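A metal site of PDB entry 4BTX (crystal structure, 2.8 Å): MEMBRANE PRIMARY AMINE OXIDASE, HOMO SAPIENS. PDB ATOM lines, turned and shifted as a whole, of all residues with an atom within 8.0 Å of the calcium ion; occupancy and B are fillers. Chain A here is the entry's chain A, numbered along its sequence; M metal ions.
The backbone NH (N) of Arg 611 sits at hydrogen-bond distance from the backbone carbonyl oxygen (O) of Asp 647, at 2.9 Å.
The side-chain amide nitrogen (ND2) of Asn 511 sits close to the backbone carbonyl oxygen (O) of Leu 504, 3.5 Å away.
The backbone carbonyl oxygen (O) of Lys 646 is in hydrogen-bond range of the backbone NH (N) of Asn 511 (2.7 Å).
The backbone NH (N) of Asp 503 lies within hydrogen-bond range of the backbone carbonyl oxygen (O) of Glu 336, 2.9 Å away.
N of Tyr 335 sits at hydrogen-bond distance from O of Asp 503 (3.0 Å).
The backbone carbonyl oxygen (O) of Val 506 lies close to the side-chain amide oxygen (OD1) of Asn 511 (3.0 Å).
The side-chain carboxylate (OD2) of Asp 503 lies within salt-bridge range of the side-chain amino group (NZ) of Lys 80 (3.2 Å).
The side-chain carboxylate of Asp 647 lies within salt-bridge range of the side-chain amino group of Lys 80 (2.6 Å).
Merely in contact with the calcium ion: Asn 511.
Six residues have an atom within 4 Å of the calcium ion: Asp 503, Leu 504, Asp 505, Asn 511, Asp 647 and Leu 648.
Along chain A the residues within 4 Å of the calcium ion span positions 503 to 648.
The calcium ion is bound by the backbone carbonyl oxygen (O) of Leu 504 (2.1 Å), the side-chain carboxylate (OD1) of Asp 647 (2.2 Å), the side-chain carboxylate (OD1) of Asp 505 (2.3 Å), the backbone carbonyl oxygen (O) of Leu 648 (2.4 Å) and the side-chain carboxylate (OD1) of Asp 503 (2.5 Å).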
ATOM      1  N   LYS A  80     -26.810  -8.340 -12.422  1.00  0.00           N
ATOM      2  CA  LYS A  80     -26.447  -7.874 -11.088  1.00  0.00           C
ATOM      3  C   LYS A  80     -27.667  -7.867 -10.152  1.00  0.00           C
ATOM      4  O   LYS A  80     -27.592  -8.352  -9.001  1.00  0.00           O
ATOM      5  CB  LYS A  80     -25.830  -6.482 -11.189  1.00  0.00           C
ATOM      6  CG  LYS A  80     -25.063  -6.033  -9.942  1.00  0.00           C
ATOM      7  CD  LYS A  80     -24.886  -4.515  -9.887  1.00  0.00           C
ATOM      8  CE  LYS A  80     -23.748  -4.141  -8.947  1.00  0.00           C
ATOM      9  NZ  LYS A  80     -23.622  -2.669  -8.757  1.00  0.00           N
ATOM     10  N   LEU A 333     -17.744  -4.030  -0.566  1.00  0.00           N
ATOM     11  CA  LEU A 333     -17.196  -2.775  -1.107  1.00  0.00           C
ATOM     12  C   LEU A 333     -17.378  -2.690  -2.617  1.00  0.00           C
ATOM     13  O   LEU A 333     -17.761  -1.649  -3.168  1.00  0.00           O
ATOM     14  CB  LEU A 333     -15.717  -2.688  -0.790  1.00  0.00           C
ATOM     15  CG  LEU A 333     -15.411  -3.141   0.658  1.00  0.00           C
ATOM     16  CD1 LEU A 333     -13.933  -3.328   0.922  1.00  0.00           C
ATOM     17  CD2 LEU A 333     -15.955  -2.118   1.629  1.00  0.00           C
ATOM     18  N   VAL A 334     -17.134  -3.830  -3.279  1.00  0.00           N
ATOM     19  CA  VAL A 334     -17.175  -3.910  -4.733  1.00  0.00           C
ATOM     20  C   VAL A 334     -17.858  -5.174  -5.193  1.00  0.00           C
ATOM     21  O   VAL A 334     -17.581  -6.260  -4.686  1.00  0.00           O
ATOM     22  CB  VAL A 334     -15.763  -3.895  -5.361  1.00  0.00           C
ATOM     23  CG1 VAL A 334     -15.429  -2.508  -5.853  1.00  0.00           C
ATOM     24  CG2 VAL A 334     -14.712  -4.358  -4.371  1.00  0.00           C
ATOM     25  N   TYR A 335     -18.740  -5.002  -6.158  1.00  0.00           N
ATOM     26  CA  TYR A 335     -19.408  -6.095  -6.820  1.00  0.00           C
ATOM     27  C   TYR A 335     -18.432  -6.814  -7.752  1.00  0.00           C
ATOM     28  O   TYR A 335     -18.396  -8.029  -7.792  1.00  0.00           O
ATOM     29  CB  TYR A 335     -20.608  -5.546  -7.594  1.00  0.00           C
ATOM     30  CG  TYR A 335     -21.347  -6.594  -8.394  1.00  0.00           C
ATOM     31  CD1 TYR A 335     -22.141  -7.548  -7.794  1.00  0.00           C
ATOM     32  CD2 TYR A 335     -21.234  -6.631  -9.762  1.00  0.00           C
ATOM     33  CE1 TYR A 335     -22.792  -8.514  -8.536  1.00  0.00           C
ATOM     34  CE2 TYR A 335     -21.890  -7.570 -10.516  1.00  0.00           C
ATOM     35  CZ  TYR A 335     -22.670  -8.524  -9.913  1.00  0.00           C
ATOM     36  OH  TYR A 335     -23.283  -9.475 -10.727  1.00  0.00           O
ATOM     37  N   GLU A 336     -17.618  -6.036  -8.472  1.00  0.00           N
ATOM     38  CA  GLU A 336     -16.662  -6.532  -9.485  1.00  0.00           C
ATOM     39  C   GLU A 336     -15.467  -5.600  -9.632  1.00  0.00           C
ATOM     40  O   GLU A 336     -15.612  -4.374  -9.690  1.00  0.00           O
ATOM     41  CB  GLU A 336     -17.362  -6.572 -10.840  1.00  0.00           C
ATOM     42  CG  GLU A 336     -16.488  -7.052 -12.006  1.00  0.00           C
ATOM     43  CD  GLU A 336     -17.147  -6.810 -13.361  1.00  0.00           C
ATOM     44  OE1 GLU A 336     -18.316  -6.359 -13.384  1.00  0.00           O
ATOM     45  OE2 GLU A 336     -16.497  -7.073 -14.401  1.00  0.00           O
ATOM     46  N   VAL A 502     -13.939  -1.076 -12.219  1.00  0.00           N
ATOM     47  CA  VAL A 502     -14.069  -1.042 -10.776  1.00  0.00           C
ATOM     48  C   VAL A 502     -15.471  -0.621 -10.400  1.00  0.00           C
ATOM     49  O   VAL A 502     -15.759   0.575 -10.329  1.00  0.00           O
ATOM     50  CB  VAL A 502     -13.082  -0.078 -10.146  1.00  0.00           C
ATOM     51  CG1 VAL A 502     -13.168  -0.183  -8.633  1.00  0.00           C
ATOM     52  CG2 VAL A 502     -11.688  -0.424 -10.616  1.00  0.00           C
ATOM     53  N   ASP A 503     -16.329  -1.613 -10.168  1.00  0.00           N
ATOM     54  CA  ASP A 503     -17.694  -1.369  -9.758  1.00  0.00           C
ATOM     55  C   ASP A 503     -17.786  -1.446  -8.256  1.00  0.00           C
ATOM     56  O   ASP A 503     -18.122  -2.489  -7.695  1.00  0.00           O
ATOM     57  CB  ASP A 503     -18.660  -2.354 -10.385  1.00  0.00           C
ATOM     58  CG  ASP A 503     -20.079  -2.111  -9.962  1.00  0.00           C
ATOM     59  OD1 ASP A 503     -20.409  -1.061  -9.338  1.00  0.00           O
ATOM     60  OD2 ASP A 503     -20.877  -3.016 -10.267  1.00  0.00           O
ATOM     61  N   LEU A 504     -17.461  -0.322  -7.645  1.00  0.00           N
ATOM     62  CA  LEU A 504     -17.769  -0.075  -6.251  1.00  0.00           C
ATOM     63  C   LEU A 504     -19.263   0.062  -6.047  1.00  0.00           C
ATOM     64  O   LEU A 504     -20.005   0.518  -6.926  1.00  0.00           O
ATOM     65  CB  LEU A 504     -17.119   1.201  -5.776  1.00  0.00           C
ATOM     66  CG  LEU A 504     -15.610   1.113  -5.625  1.00  0.00           C
ATOM     67  CD1 LEU A 504     -14.914   2.381  -6.112  1.00  0.00           C
ATOM     68  CD2 LEU A 504     -15.277   0.826  -4.172  1.00  0.00           C
ATOM     69  N   ASP A 505     -19.665  -0.364  -4.869  1.00  0.00           N
ATOM     70  CA  ASP A 505     -21.001  -0.169  -4.395  1.00  0.00           C
ATOM     71  C   ASP A 505     -20.780   0.264  -2.972  1.00  0.00           C
ATOM     72  O   ASP A 505     -20.783  -0.574  -2.056  1.00  0.00           O
ATOM     73  CB  ASP A 505     -21.810  -1.477  -4.448  1.00  0.00           C
ATOM     74  CG  ASP A 505     -22.258  -1.829  -5.858  1.00  0.00           C
ATOM     75  OD1 ASP A 505     -22.132  -0.966  -6.775  1.00  0.00           O
ATOM     76  OD2 ASP A 505     -22.718  -2.983  -6.049  1.00  0.00           O
ATOM     77  N   VAL A 506     -20.547   1.571  -2.805  1.00  0.00           N
ATOM     78  CA  VAL A 506     -20.124   2.065  -1.517  1.00  0.00           C
ATOM     79  C   VAL A 506     -21.308   2.208  -0.579  1.00  0.00           C
ATOM     80  O   VAL A 506     -22.194   3.039  -0.813  1.00  0.00           O
ATOM     81  CB  VAL A 506     -19.353   3.382  -1.588  1.00  0.00           C
ATOM     82  CG1 VAL A 506     -18.858   3.779  -0.194  1.00  0.00           C
ATOM     83  CG2 VAL A 506     -18.173   3.218  -2.504  1.00  0.00           C
ATOM     84  N   GLY A 508     -23.852   0.442  -0.367  1.00  0.00           N
ATOM     85  CA  GLY A 508     -25.006   0.435  -1.246  1.00  0.00           C
ATOM     86  C   GLY A 508     -24.768   0.791  -2.694  1.00  0.00           C
ATOM     87  O   GLY A 508     -23.704   1.218  -3.096  1.00  0.00           O
ATOM     88  N   LEU A 509     -25.793   0.619  -3.495  1.00  0.00           N
ATOM     89  CA  LEU A 509     -25.658   0.857  -4.903  1.00  0.00           C
ATOM     90  C   LEU A 509     -25.512   2.292  -5.229  1.00  0.00           C
ATOM     91  O   LEU A 509     -24.745   2.660  -6.124  1.00  0.00           O
ATOM     92  CB  LEU A 509     -26.892   0.344  -5.634  1.00  0.00           C
ATOM     93  CG  LEU A 509     -26.671  -0.921  -6.417  1.00  0.00           C
ATOM     94  CD1 LEU A 509     -26.138  -2.044  -5.528  1.00  0.00           C
ATOM     95  CD2 LEU A 509     -27.984  -1.259  -7.089  1.00  0.00           C
ATOM     96  N   GLU A 510     -26.263   3.120  -4.532  1.00  0.00           N
ATOM     97  CA  GLU A 510     -26.411   4.505  -4.938  1.00  0.00           C
ATOM     98  C   GLU A 510     -25.189   5.247  -4.420  1.00  0.00           C
ATOM     99  O   GLU A 510     -24.862   5.224  -3.208  1.00  0.00           O
ATOM    100  CB  GLU A 510     -27.757   5.078  -4.493  1.00  0.00           C
ATOM    101  CG  GLU A 510     -28.951   4.192  -4.907  1.00  0.00           C
ATOM    102  CD  GLU A 510     -29.340   3.054  -3.908  1.00  0.00           C
ATOM    103  OE1 GLU A 510     -28.922   3.025  -2.711  1.00  0.00           O
ATOM    104  OE2 GLU A 510     -30.096   2.142  -4.334  1.00  0.00           O
ATOM    105  N   ASN A 511     -24.446   5.792  -5.370  1.00  0.00           N
ATOM    106  CA  ASN A 511     -23.230   6.485  -5.085  1.00  0.00           C
ATOM    107  C   ASN A 511     -23.237   7.828  -5.801  1.00  0.00           C
ATOM    108  O   ASN A 511     -23.856   8.000  -6.876  1.00  0.00           O
ATOM    109  CB  ASN A 511     -22.016   5.677  -5.551  1.00  0.00           C
ATOM    110  CG  ASN A 511     -21.825   4.374  -4.784  1.00  0.00           C
ATOM    111  OD1 ASN A 511     -21.838   4.344  -3.538  1.00  0.00           O
ATOM    112  ND2 ASN A 511     -21.616   3.266  -5.550  1.00  0.00           N
ATOM    113  N   LEU A 563     -15.789   7.861  -4.576  1.00  0.00           N
ATOM    114  CA  LEU A 563     -17.218   7.605  -4.658  1.00  0.00           C
ATOM    115  C   LEU A 563     -17.667   7.451  -3.240  1.00  0.00           C
ATOM    116  O   LEU A 563     -16.959   6.864  -2.399  1.00  0.00           O
ATOM    117  CB  LEU A 563     -17.568   6.332  -5.410  1.00  0.00           C
ATOM    118  CG  LEU A 563     -16.865   5.876  -6.690  1.00  0.00           C
ATOM    119  CD1 LEU A 563     -17.810   5.056  -7.578  1.00  0.00           C
ATOM    120  CD2 LEU A 563     -16.309   7.030  -7.494  1.00  0.00           C
ATOM    121  N   THR A 609     -19.022   6.171 -14.789  1.00  0.00           N
ATOM    122  CA  THR A 609     -20.144   5.957 -15.640  1.00  0.00           C
ATOM    123  C   THR A 609     -21.216   5.256 -14.836  1.00  0.00           C
ATOM    124  O   THR A 609     -20.912   4.497 -13.903  1.00  0.00           O
ATOM    125  CB  THR A 609     -19.657   5.138 -16.854  1.00  0.00           C
ATOM    126  OG1 THR A 609     -19.345   6.047 -17.925  1.00  0.00           O
ATOM    127  CG2 THR A 609     -20.682   4.105 -17.342  1.00  0.00           C
ATOM    128  N   GLN A 610     -22.475   5.555 -15.175  1.00  0.00           N
ATOM    129  CA  GLN A 610     -23.637   4.723 -14.780  1.00  0.00           C
ATOM    130  C   GLN A 610     -23.445   3.278 -15.200  1.00  0.00           C
ATOM    131  O   GLN A 610     -23.254   3.019 -16.426  1.00  0.00           O
ATOM    132  CB  GLN A 610     -24.918   5.217 -15.454  1.00  0.00           C
ATOM    133  CG  GLN A 610     -25.706   6.238 -14.656  1.00  0.00           C
ATOM    134  CD  GLN A 610     -27.041   6.561 -15.304  1.00  0.00           C
ATOM    135  OE1 GLN A 610     -27.687   5.682 -15.875  1.00  0.00           O
ATOM    136  NE2 GLN A 610     -27.467   7.817 -15.202  1.00  0.00           N
ATOM    137  N   ARG A 611     -23.517   2.352 -14.230  1.00  0.00           N
ATOM    138  CA  ARG A 611     -23.370   0.901 -14.478  1.00  0.00           C
ATOM    139  C   ARG A 611     -24.479   0.407 -15.317  1.00  0.00           C
ATOM    140  O   ARG A 611     -25.561   0.919 -15.212  1.00  0.00           O
ATOM    141  CB  ARG A 611     -23.429   0.082 -13.206  1.00  0.00           C
ATOM    142  CG  ARG A 611     -22.417  -1.037 -13.210  1.00  0.00           C
ATOM    143  CD  ARG A 611     -22.929  -2.336 -12.635  1.00  0.00           C
ATOM    144  NE  ARG A 611     -23.833  -3.017 -13.550  1.00  0.00           N
ATOM    145  CZ  ARG A 611     -23.903  -4.348 -13.701  1.00  0.00           C
ATOM    146  NH1 ARG A 611     -23.097  -5.175 -13.035  1.00  0.00           N
ATOM    147  NH2 ARG A 611     -24.807  -4.851 -14.547  1.00  0.00           N
ATOM    148  N   LYS A 646     -26.528   7.278  -8.373  1.00  0.00           N
ATOM    149  CA  LYS A 646     -26.864   6.048  -9.093  1.00  0.00           C
ATOM    150  C   LYS A 646     -25.906   4.922  -8.753  1.00  0.00           C
ATOM    151  O   LYS A 646     -25.031   5.063  -7.895  1.00  0.00           O
ATOM    152  CB  LYS A 646     -26.880   6.273 -10.603  1.00  0.00           C
ATOM    153  CG  LYS A 646     -27.453   7.599 -11.051  1.00  0.00           C
ATOM    154  CD  LYS A 646     -28.834   7.891 -10.508  1.00  0.00           C
ATOM    155  CE  LYS A 646     -29.901   7.017 -11.136  1.00  0.00           C
ATOM    156  NZ  LYS A 646     -29.996   7.327 -12.583  1.00  0.00           N
ATOM    157  N   ASP A 647     -26.102   3.782  -9.422  1.00  0.00           N
ATOM    158  CA  ASP A 647     -25.110   2.694  -9.401  1.00  0.00           C
ATOM    159  C   ASP A 647     -24.002   3.103 -10.330  1.00  0.00           C
ATOM    160  O   ASP A 647     -24.220   3.216 -11.546  1.00  0.00           O
ATOM    161  CB  ASP A 647     -25.697   1.355  -9.868  1.00  0.00           C
ATOM    162  CG  ASP A 647     -24.745   0.186  -9.630  1.00  0.00           C
ATOM    163  OD1 ASP A 647     -23.540   0.391  -9.317  1.00  0.00           O
ATOM    164  OD2 ASP A 647     -25.227  -0.952  -9.786  1.00  0.00           O
ATOM    165  N   LEU A 648     -22.843   3.332  -9.743  1.00  0.00           N
ATOM    166  CA  LEU A 648     -21.738   3.882 -10.501  1.00  0.00           C
ATOM    167  C   LEU A 648     -20.653   2.851 -10.703  1.00  0.00           C
ATOM    168  O   LEU A 648     -20.404   2.007  -9.815  1.00  0.00           O
ATOM    169  CB  LEU A 648     -21.145   5.074  -9.760  1.00  0.00           C
ATOM    170  CG  LEU A 648     -22.055   6.266  -9.530  1.00  0.00           C
ATOM    171  CD1 LEU A 648     -21.249   7.296  -8.772  1.00  0.00           C
ATOM    172  CD2 LEU A 648     -22.630   6.857 -10.810  1.00  0.00           C
ATOM    173  N   VAL A 649     -20.001   2.929 -11.859  1.00  0.00           N
ATOM    174  CA  VAL A 649     -18.790   2.142 -12.084  1.00  0.00           C
ATOM    175  C   VAL A 649     -17.671   3.037 -12.578  1.00  0.00           C
ATOM    176  O   VAL A 649     -17.867   3.872 -13.482  1.00  0.00           O
ATOM    177  CB  VAL A 649     -19.016   0.918 -13.009  1.00  0.00           C
ATOM    178  CG1 VAL A 649     -19.540   1.325 -14.383  1.00  0.00           C
ATOM    179  CG2 VAL A 649     -17.732   0.111 -13.100  1.00  0.00           C
ATOM    180  N   ALA A 650     -16.520   2.859 -11.948  1.00  0.00           N
ATOM    181  CA  ALA A 650     -15.337   3.601 -12.237  1.00  0.00           C
ATOM    182  C   ALA A 650     -14.441   2.758 -13.134  1.00  0.00           C
ATOM    183  O   ALA A 650     -14.107   1.620 -12.792  1.00  0.00           O
ATOM    184  CB  ALA A 650     -14.614   3.921 -10.959  1.00  0.00           C
HETATM  185 CA    CA M   1     -21.669   0.810  -8.188  1.00  0.00          CA
